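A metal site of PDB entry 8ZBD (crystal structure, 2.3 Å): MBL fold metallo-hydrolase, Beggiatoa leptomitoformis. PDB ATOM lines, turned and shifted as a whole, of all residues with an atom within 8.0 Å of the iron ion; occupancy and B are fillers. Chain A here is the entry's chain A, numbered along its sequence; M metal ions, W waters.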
ATOM      1  N   THR A  13      -7.096  17.458 -17.532  1.00  0.00           N
ATOM      2  CA  THR A  13      -8.147  17.791 -18.480  1.00  0.00           C
ATOM      3  C   THR A  13      -8.146  16.824 -19.656  1.00  0.00           C
ATOM      4  O   THR A  13      -7.078  16.436 -20.149  1.00  0.00           O
ATOM      5  CB  THR A  13      -7.961  19.226 -18.991  1.00  0.00           C
ATOM      6  OG1 THR A  13      -7.924  20.104 -17.868  1.00  0.00           O
ATOM      7  CG2 THR A  13      -9.120  19.649 -19.893  1.00  0.00           C
ATOM      8  N   ASP A  30     -12.181  21.913 -25.390  1.00  0.00           N
ATOM      9  CA  ASP A  30     -11.326  22.196 -24.245  1.00  0.00           C
ATOM     10  C   ASP A  30      -9.843  21.936 -24.500  1.00  0.00           C
ATOM     11  O   ASP A  30      -9.197  21.167 -23.779  1.00  0.00           O
ATOM     12  CB  ASP A  30     -11.817  21.415 -23.022  1.00  0.00           C
ATOM     13  CG  ASP A  30     -13.163  21.948 -22.477  1.00  0.00           C
ATOM     14  OD1 ASP A  30     -13.492  23.139 -22.705  1.00  0.00           O
ATOM     15  OD2 ASP A  30     -13.881  21.176 -21.810  1.00  0.00           O
ATOM     16  N   THR A  56     -16.131  24.279 -22.993  1.00  0.00           N
ATOM     17  CA  THR A  56     -17.319  24.029 -22.188  1.00  0.00           C
ATOM     18  C   THR A  56     -17.616  25.177 -21.221  1.00  0.00           C
ATOM     19  O   THR A  56     -18.781  25.432 -20.890  1.00  0.00           O
ATOM     20  CB  THR A  56     -17.156  22.728 -21.401  1.00  0.00           C
ATOM     21  OG1 THR A  56     -15.965  22.827 -20.604  1.00  0.00           O
ATOM     22  CG2 THR A  56     -17.013  21.526 -22.370  1.00  0.00           C
ATOM     23  N   HIS A  57     -16.581  25.877 -20.765  1.00  0.00           N
ATOM     24  CA  HIS A  57     -16.757  26.952 -19.800  1.00  0.00           C
ATOM     25  C   HIS A  57     -15.434  27.699 -19.638  1.00  0.00           C
ATOM     26  O   HIS A  57     -14.419  27.339 -20.232  1.00  0.00           O
ATOM     27  CB  HIS A  57     -17.292  26.412 -18.459  1.00  0.00           C
ATOM     28  CG  HIS A  57     -16.351  25.497 -17.758  1.00  0.00           C
ATOM     29  ND1 HIS A  57     -16.081  24.212 -18.190  1.00  0.00           N
ATOM     30  CD2 HIS A  57     -15.641  25.654 -16.605  1.00  0.00           C
ATOM     31  CE1 HIS A  57     -15.249  23.628 -17.352  1.00  0.00           C
ATOM     32  NE2 HIS A  57     -14.958  24.476 -16.385  1.00  0.00           N
ATOM     33  N   ILE A  58     -15.467  28.747 -18.828  1.00  0.00           N
ATOM     34  CA  ILE A  58     -14.279  29.518 -18.480  1.00  0.00           C
ATOM     35  C   ILE A  58     -13.544  28.718 -17.401  1.00  0.00           C
ATOM     36  O   ILE A  58     -13.974  28.662 -16.246  1.00  0.00           O
ATOM     37  CB  ILE A  58     -14.660  30.921 -17.997  1.00  0.00           C
ATOM     38  CG1 ILE A  58     -15.385  31.676 -19.113  1.00  0.00           C
ATOM     39  CG2 ILE A  58     -13.456  31.694 -17.515  1.00  0.00           C
ATOM     40  CD1 ILE A  58     -14.711  31.503 -20.468  1.00  0.00           C
ATOM     41  N   HIS A  59     -12.426  28.096 -17.786  1.00  0.00           N
ATOM     42  CA  HIS A  59     -11.732  27.158 -16.916  1.00  0.00           C
ATOM     43  C   HIS A  59     -10.983  27.880 -15.809  1.00  0.00           C
ATOM     44  O   HIS A  59     -10.391  28.933 -16.024  1.00  0.00           O
ATOM     45  CB  HIS A  59     -10.761  26.314 -17.736  1.00  0.00           C
ATOM     46  CG  HIS A  59     -11.442  25.455 -18.747  1.00  0.00           C
ATOM     47  ND1 HIS A  59     -12.125  24.310 -18.413  1.00  0.00           N
ATOM     48  CD2 HIS A  59     -11.616  25.610 -20.079  1.00  0.00           C
ATOM     49  CE1 HIS A  59     -12.660  23.779 -19.490  1.00  0.00           C
ATOM     50  NE2 HIS A  59     -12.371  24.551 -20.519  1.00  0.00           N
ATOM     51  N   ALA A  60     -11.012  27.305 -14.605  1.00  0.00           N
ATOM     52  CA  ALA A  60     -10.295  27.875 -13.475  1.00  0.00           C
ATOM     53  C   ALA A  60      -8.971  27.175 -13.205  1.00  0.00           C
ATOM     54  O   ALA A  60      -8.150  27.715 -12.448  1.00  0.00           O
ATOM     55  CB  ALA A  60     -11.162  27.818 -12.204  1.00  0.00           C
ATOM     56  N   ASP A  61      -8.741  26.013 -13.814  1.00  0.00           N
ATOM     57  CA  ASP A  61      -7.608  25.172 -13.481  1.00  0.00           C
ATOM     58  C   ASP A  61      -6.519  25.149 -14.543  1.00  0.00           C
ATOM     59  O   ASP A  61      -5.419  24.668 -14.255  1.00  0.00           O
ATOM     60  CB  ASP A  61      -8.077  23.727 -13.249  1.00  0.00           C
ATOM     61  CG  ASP A  61      -8.726  23.123 -14.500  1.00  0.00           C
ATOM     62  OD1 ASP A  61      -9.743  23.679 -14.992  1.00  0.00           O
ATOM     63  OD2 ASP A  61      -8.211  22.114 -15.020  1.00  0.00           O
ATOM     64  N   HIS A  62      -6.804  25.588 -15.765  1.00  0.00           N
ATOM     65  CA  HIS A  62      -5.801  25.602 -16.818  1.00  0.00           C
ATOM     66  C   HIS A  62      -6.123  26.758 -17.743  1.00  0.00           C
ATOM     67  O   HIS A  62      -7.233  27.304 -17.726  1.00  0.00           O
ATOM     68  CB  HIS A  62      -5.763  24.264 -17.594  1.00  0.00           C
ATOM     69  CG  HIS A  62      -6.993  24.018 -18.408  1.00  0.00           C
ATOM     70  ND1 HIS A  62      -8.058  23.276 -17.948  1.00  0.00           N
ATOM     71  CD2 HIS A  62      -7.354  24.438 -19.651  1.00  0.00           C
ATOM     72  CE1 HIS A  62      -9.012  23.240 -18.857  1.00  0.00           C
ATOM     73  NE2 HIS A  62      -8.610  23.939 -19.899  1.00  0.00           N
ATOM     74  N   HIS A 113     -21.556  24.447 -12.091  1.00  0.00           N
ATOM     75  CA  HIS A 113     -20.131  24.581 -11.828  1.00  0.00           C
ATOM     76  C   HIS A 113     -19.683  26.020 -12.042  1.00  0.00           C
ATOM     77  O   HIS A 113     -19.021  26.614 -11.188  1.00  0.00           O
ATOM     78  CB  HIS A 113     -19.357  23.607 -12.727  1.00  0.00           C
ATOM     79  CG  HIS A 113     -17.870  23.726 -12.644  1.00  0.00           C
ATOM     80  ND1 HIS A 113     -17.159  23.425 -11.505  1.00  0.00           N
ATOM     81  CD2 HIS A 113     -16.950  24.037 -13.584  1.00  0.00           C
ATOM     82  CE1 HIS A 113     -15.864  23.563 -11.740  1.00  0.00           C
ATOM     83  NE2 HIS A 113     -15.721  23.939 -12.999  1.00  0.00           N
ATOM     84  N   THR A 114     -20.067  26.607 -13.188  1.00  0.00           N
ATOM     85  CA  THR A 114     -20.084  28.050 -13.420  1.00  0.00           C
ATOM     86  C   THR A 114     -21.464  28.419 -13.983  1.00  0.00           C
ATOM     87  O   THR A 114     -22.291  27.539 -14.258  1.00  0.00           O
ATOM     88  CB  THR A 114     -19.006  28.507 -14.414  1.00  0.00           C
ATOM     89  OG1 THR A 114     -19.271  27.946 -15.698  1.00  0.00           O
ATOM     90  CG2 THR A 114     -17.629  28.091 -13.951  1.00  0.00           C
ATOM     91  N   HIS A 117     -21.725  27.429 -18.032  1.00  0.00           N
ATOM     92  CA  HIS A 117     -21.260  26.111 -18.453  1.00  0.00           C
ATOM     93  C   HIS A 117     -22.192  25.472 -19.480  1.00  0.00           C
ATOM     94  O   HIS A 117     -23.416  25.371 -19.284  1.00  0.00           O
ATOM     95  CB  HIS A 117     -21.102  25.194 -17.238  1.00  0.00           C
ATOM     96  CG  HIS A 117     -20.485  23.873 -17.556  1.00  0.00           C
ATOM     97  ND1 HIS A 117     -21.224  22.815 -18.056  1.00  0.00           N
ATOM     98  CD2 HIS A 117     -19.208  23.427 -17.462  1.00  0.00           C
ATOM     99  CE1 HIS A 117     -20.415  21.780 -18.250  1.00  0.00           C
ATOM    100  NE2 HIS A 117     -19.190  22.125 -17.898  1.00  0.00           N
ATOM    101  N   GLY A 133     -18.126  18.273 -19.896  1.00  0.00           N
ATOM    102  CA  GLY A 133     -17.327  19.285 -19.236  1.00  0.00           C
ATOM    103  C   GLY A 133     -17.201  19.000 -17.767  1.00  0.00           C
ATOM    104  O   GLY A 133     -17.023  17.867 -17.338  1.00  0.00           O
ATOM    105  N   ASP A 134     -17.324  20.034 -16.957  1.00  0.00           N
ATOM    106  CA  ASP A 134     -17.317  19.838 -15.524  1.00  0.00           C
ATOM    107  C   ASP A 134     -18.715  19.814 -14.933  1.00  0.00           C
ATOM    108  O   ASP A 134     -18.897  20.172 -13.761  1.00  0.00           O
ATOM    109  CB  ASP A 134     -16.457  20.920 -14.858  1.00  0.00           C
ATOM    110  CG  ASP A 134     -14.984  20.668 -15.040  1.00  0.00           C
ATOM    111  OD1 ASP A 134     -14.593  19.493 -15.129  1.00  0.00           O
ATOM    112  OD2 ASP A 134     -14.215  21.644 -15.111  1.00  0.00           O
ATOM    113  N   ALA A 135     -19.727  19.434 -15.721  1.00  0.00           N
ATOM    114  CA  ALA A 135     -21.060  19.309 -15.141  1.00  0.00           C
ATOM    115  C   ALA A 135     -21.220  17.936 -14.475  1.00  0.00           C
ATOM    116  O   ALA A 135     -21.234  17.831 -13.253  1.00  0.00           O
ATOM    117  CB  ALA A 135     -22.134  19.523 -16.202  1.00  0.00           C
ATOM    118  N   LEU A 137     -19.277  14.372 -13.922  1.00  0.00           N
ATOM    119  CA  LEU A 137     -17.977  13.727 -13.980  1.00  0.00           C
ATOM    120  C   LEU A 137     -18.171  12.256 -13.638  1.00  0.00           C
ATOM    121  O   LEU A 137     -19.236  11.834 -13.196  1.00  0.00           O
ATOM    122  CB  LEU A 137     -16.970  14.389 -13.024  1.00  0.00           C
ATOM    123  CG  LEU A 137     -16.543  15.821 -13.414  1.00  0.00           C
ATOM    124  CD1 LEU A 137     -15.678  16.488 -12.368  1.00  0.00           C
ATOM    125  CD2 LEU A 137     -15.834  15.823 -14.748  1.00  0.00           C
ATOM    126  N   GLY A 142     -18.703  18.397 -11.036  1.00  0.00           N
ATOM    127  CA  GLY A 142     -17.841  19.556 -10.876  1.00  0.00           C
ATOM    128  C   GLY A 142     -17.997  20.162  -9.498  1.00  0.00           C
ATOM    129  O   GLY A 142     -19.065  20.082  -8.888  1.00  0.00           O
ATOM    130  N   ARG A 143     -16.921  20.737  -8.988  1.00  0.00           N
ATOM    131  CA  ARG A 143     -17.016  21.406  -7.696  1.00  0.00           C
ATOM    132  C   ARG A 143     -17.986  22.583  -7.788  1.00  0.00           C
ATOM    133  O   ARG A 143     -18.122  23.212  -8.834  1.00  0.00           O
ATOM    134  CB  ARG A 143     -15.636  21.884  -7.248  1.00  0.00           C
ATOM    135  CG  ARG A 143     -14.935  22.802  -8.229  1.00  0.00           C
ATOM    136  CD  ARG A 143     -13.463  22.887  -7.868  1.00  0.00           C
ATOM    137  NE  ARG A 143     -13.299  23.391  -6.511  1.00  0.00           N
ATOM    138  CZ  ARG A 143     -12.178  23.331  -5.807  1.00  0.00           C
ATOM    139  NH1 ARG A 143     -11.088  22.771  -6.296  1.00  0.00           N
ATOM    140  NH2 ARG A 143     -12.155  23.854  -4.580  1.00  0.00           N
ATOM    141  N   PHE A 146     -16.806  27.495  -6.099  1.00  0.00           N
ATOM    142  CA  PHE A 146     -16.399  28.767  -6.670  1.00  0.00           C
ATOM    143  C   PHE A 146     -17.488  29.804  -6.428  1.00  0.00           C
ATOM    144  O   PHE A 146     -18.551  29.509  -5.874  1.00  0.00           O
ATOM    145  CB  PHE A 146     -16.131  28.626  -8.165  1.00  0.00           C
ATOM    146  CG  PHE A 146     -14.960  27.741  -8.518  1.00  0.00           C
ATOM    147  CD1 PHE A 146     -13.867  27.624  -7.673  1.00  0.00           C
ATOM    148  CD2 PHE A 146     -14.952  27.046  -9.730  1.00  0.00           C
ATOM    149  CE1 PHE A 146     -12.798  26.815  -8.022  1.00  0.00           C
ATOM    150  CE2 PHE A 146     -13.884  26.249 -10.086  1.00  0.00           C
ATOM    151  CZ  PHE A 146     -12.801  26.129  -9.233  1.00  0.00           C
ATOM    152  N   GLY A 174     -14.941  16.358 -18.602  1.00  0.00           N
ATOM    153  CA  GLY A 174     -13.919  17.392 -18.743  1.00  0.00           C
ATOM    154  C   GLY A 174     -12.634  17.065 -18.008  1.00  0.00           C
ATOM    155  O   GLY A 174     -11.549  17.476 -18.430  1.00  0.00           O
ATOM    156  N   HIS A 175     -12.735  16.294 -16.933  1.00  0.00           N
ATOM    157  CA  HIS A 175     -11.589  15.953 -16.111  1.00  0.00           C
ATOM    158  C   HIS A 175     -11.791  14.554 -15.584  1.00  0.00           C
ATOM    159  O   HIS A 175     -12.917  14.060 -15.536  1.00  0.00           O
ATOM    160  CB  HIS A 175     -11.409  16.924 -14.919  1.00  0.00           C
ATOM    161  CG  HIS A 175     -11.142  18.332 -15.306  1.00  0.00           C
ATOM    162  ND1 HIS A 175     -12.148  19.213 -15.642  1.00  0.00           N
ATOM    163  CD2 HIS A 175      -9.978  19.032 -15.399  1.00  0.00           C
ATOM    164  CE1 HIS A 175     -11.617  20.400 -15.932  1.00  0.00           C
ATOM    165  NE2 HIS A 175     -10.311  20.310 -15.797  1.00  0.00           N
ATOM    166  N   TYR A 177      -9.441  12.220 -12.294  1.00  0.00           N
ATOM    167  CA  TYR A 177      -8.249  12.212 -11.463  1.00  0.00           C
ATOM    168  C   TYR A 177      -7.838  10.804 -11.071  1.00  0.00           C
ATOM    169  O   TYR A 177      -6.870  10.642 -10.325  1.00  0.00           O
ATOM    170  CB  TYR A 177      -8.476  13.061 -10.204  1.00  0.00           C
ATOM    171  CG  TYR A 177      -8.833  14.483 -10.560  1.00  0.00           C
ATOM    172  CD1 TYR A 177      -7.851  15.432 -10.789  1.00  0.00           C
ATOM    173  CD2 TYR A 177     -10.156  14.871 -10.728  1.00  0.00           C
ATOM    174  CE1 TYR A 177      -8.170  16.726 -11.142  1.00  0.00           C
ATOM    175  CE2 TYR A 177     -10.483  16.154 -11.084  1.00  0.00           C
ATOM    176  CZ  TYR A 177      -9.482  17.093 -11.293  1.00  0.00           C
ATOM    177  OH  TYR A 177      -9.794  18.408 -11.643  1.00  0.00           O
ATOM    178  N   PRO A 216      -7.836  25.232  -7.359  1.00  0.00           N
ATOM    179  CA  PRO A 216      -6.822  24.977  -8.383  1.00  0.00           C
ATOM    180  C   PRO A 216      -5.724  26.030  -8.302  1.00  0.00           C
ATOM    181  O   PRO A 216      -5.998  27.213  -8.079  1.00  0.00           O
ATOM    182  CB  PRO A 216      -7.594  25.053  -9.717  1.00  0.00           C
ATOM    183  CG  PRO A 216      -9.007  25.342  -9.381  1.00  0.00           C
ATOM    184  CD  PRO A 216      -9.175  25.513  -7.912  1.00  0.00           C
HETATM  185 FE    FE M   1     -13.875  23.578 -14.449  1.00  0.00          FE
HETATM  186  O   HOH W   1     -12.676  25.243 -13.516  1.00  0.00           O
HETATM  187  O   HOH W   2     -12.224  23.615 -15.820  1.00  0.00           O
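The backbone carbonyl oxygen (O) of His 57 sits close to a ring nitrogen (NE2) of His 59 (3.5 Å). ND1 of His 113 sits at hydrogen-bond distance from O of Arg 143 (2.8 Å). The backbone NH (N) of Gly 142 sits close to the backbone carbonyl oxygen (O) of Asp 134 (3.3 Å). A ring nitrogen (ND1) of His 175 is in hydrogen-bond range of the side-chain carboxylate (OD1) of Asp 134 (2.5 Å). A ring nitrogen (ND1) of His 57 lies within hydrogen-bond range of the side-chain hydroxyl (OG1) of Thr 56 (2.8 Å). The backbone NH (N) of Asp 134 sits at hydrogen-bond distance from a ring nitrogen (NE2) of His 117 (3.0 Å).
The nearest printed residue that does not touch the iron ion is Asp 61 (4.2 Å).
The iron ion is bound by OD2 of Asp 134, water W2, water W1, NE2 of His 113 and NE2 of His 57.
Water W2 lies within hydrogen-bond range of the side-chain carboxylate of Asp 61 (2.6 Å) and a ring nitrogen (ND1) of His 59 (2.7 Å).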
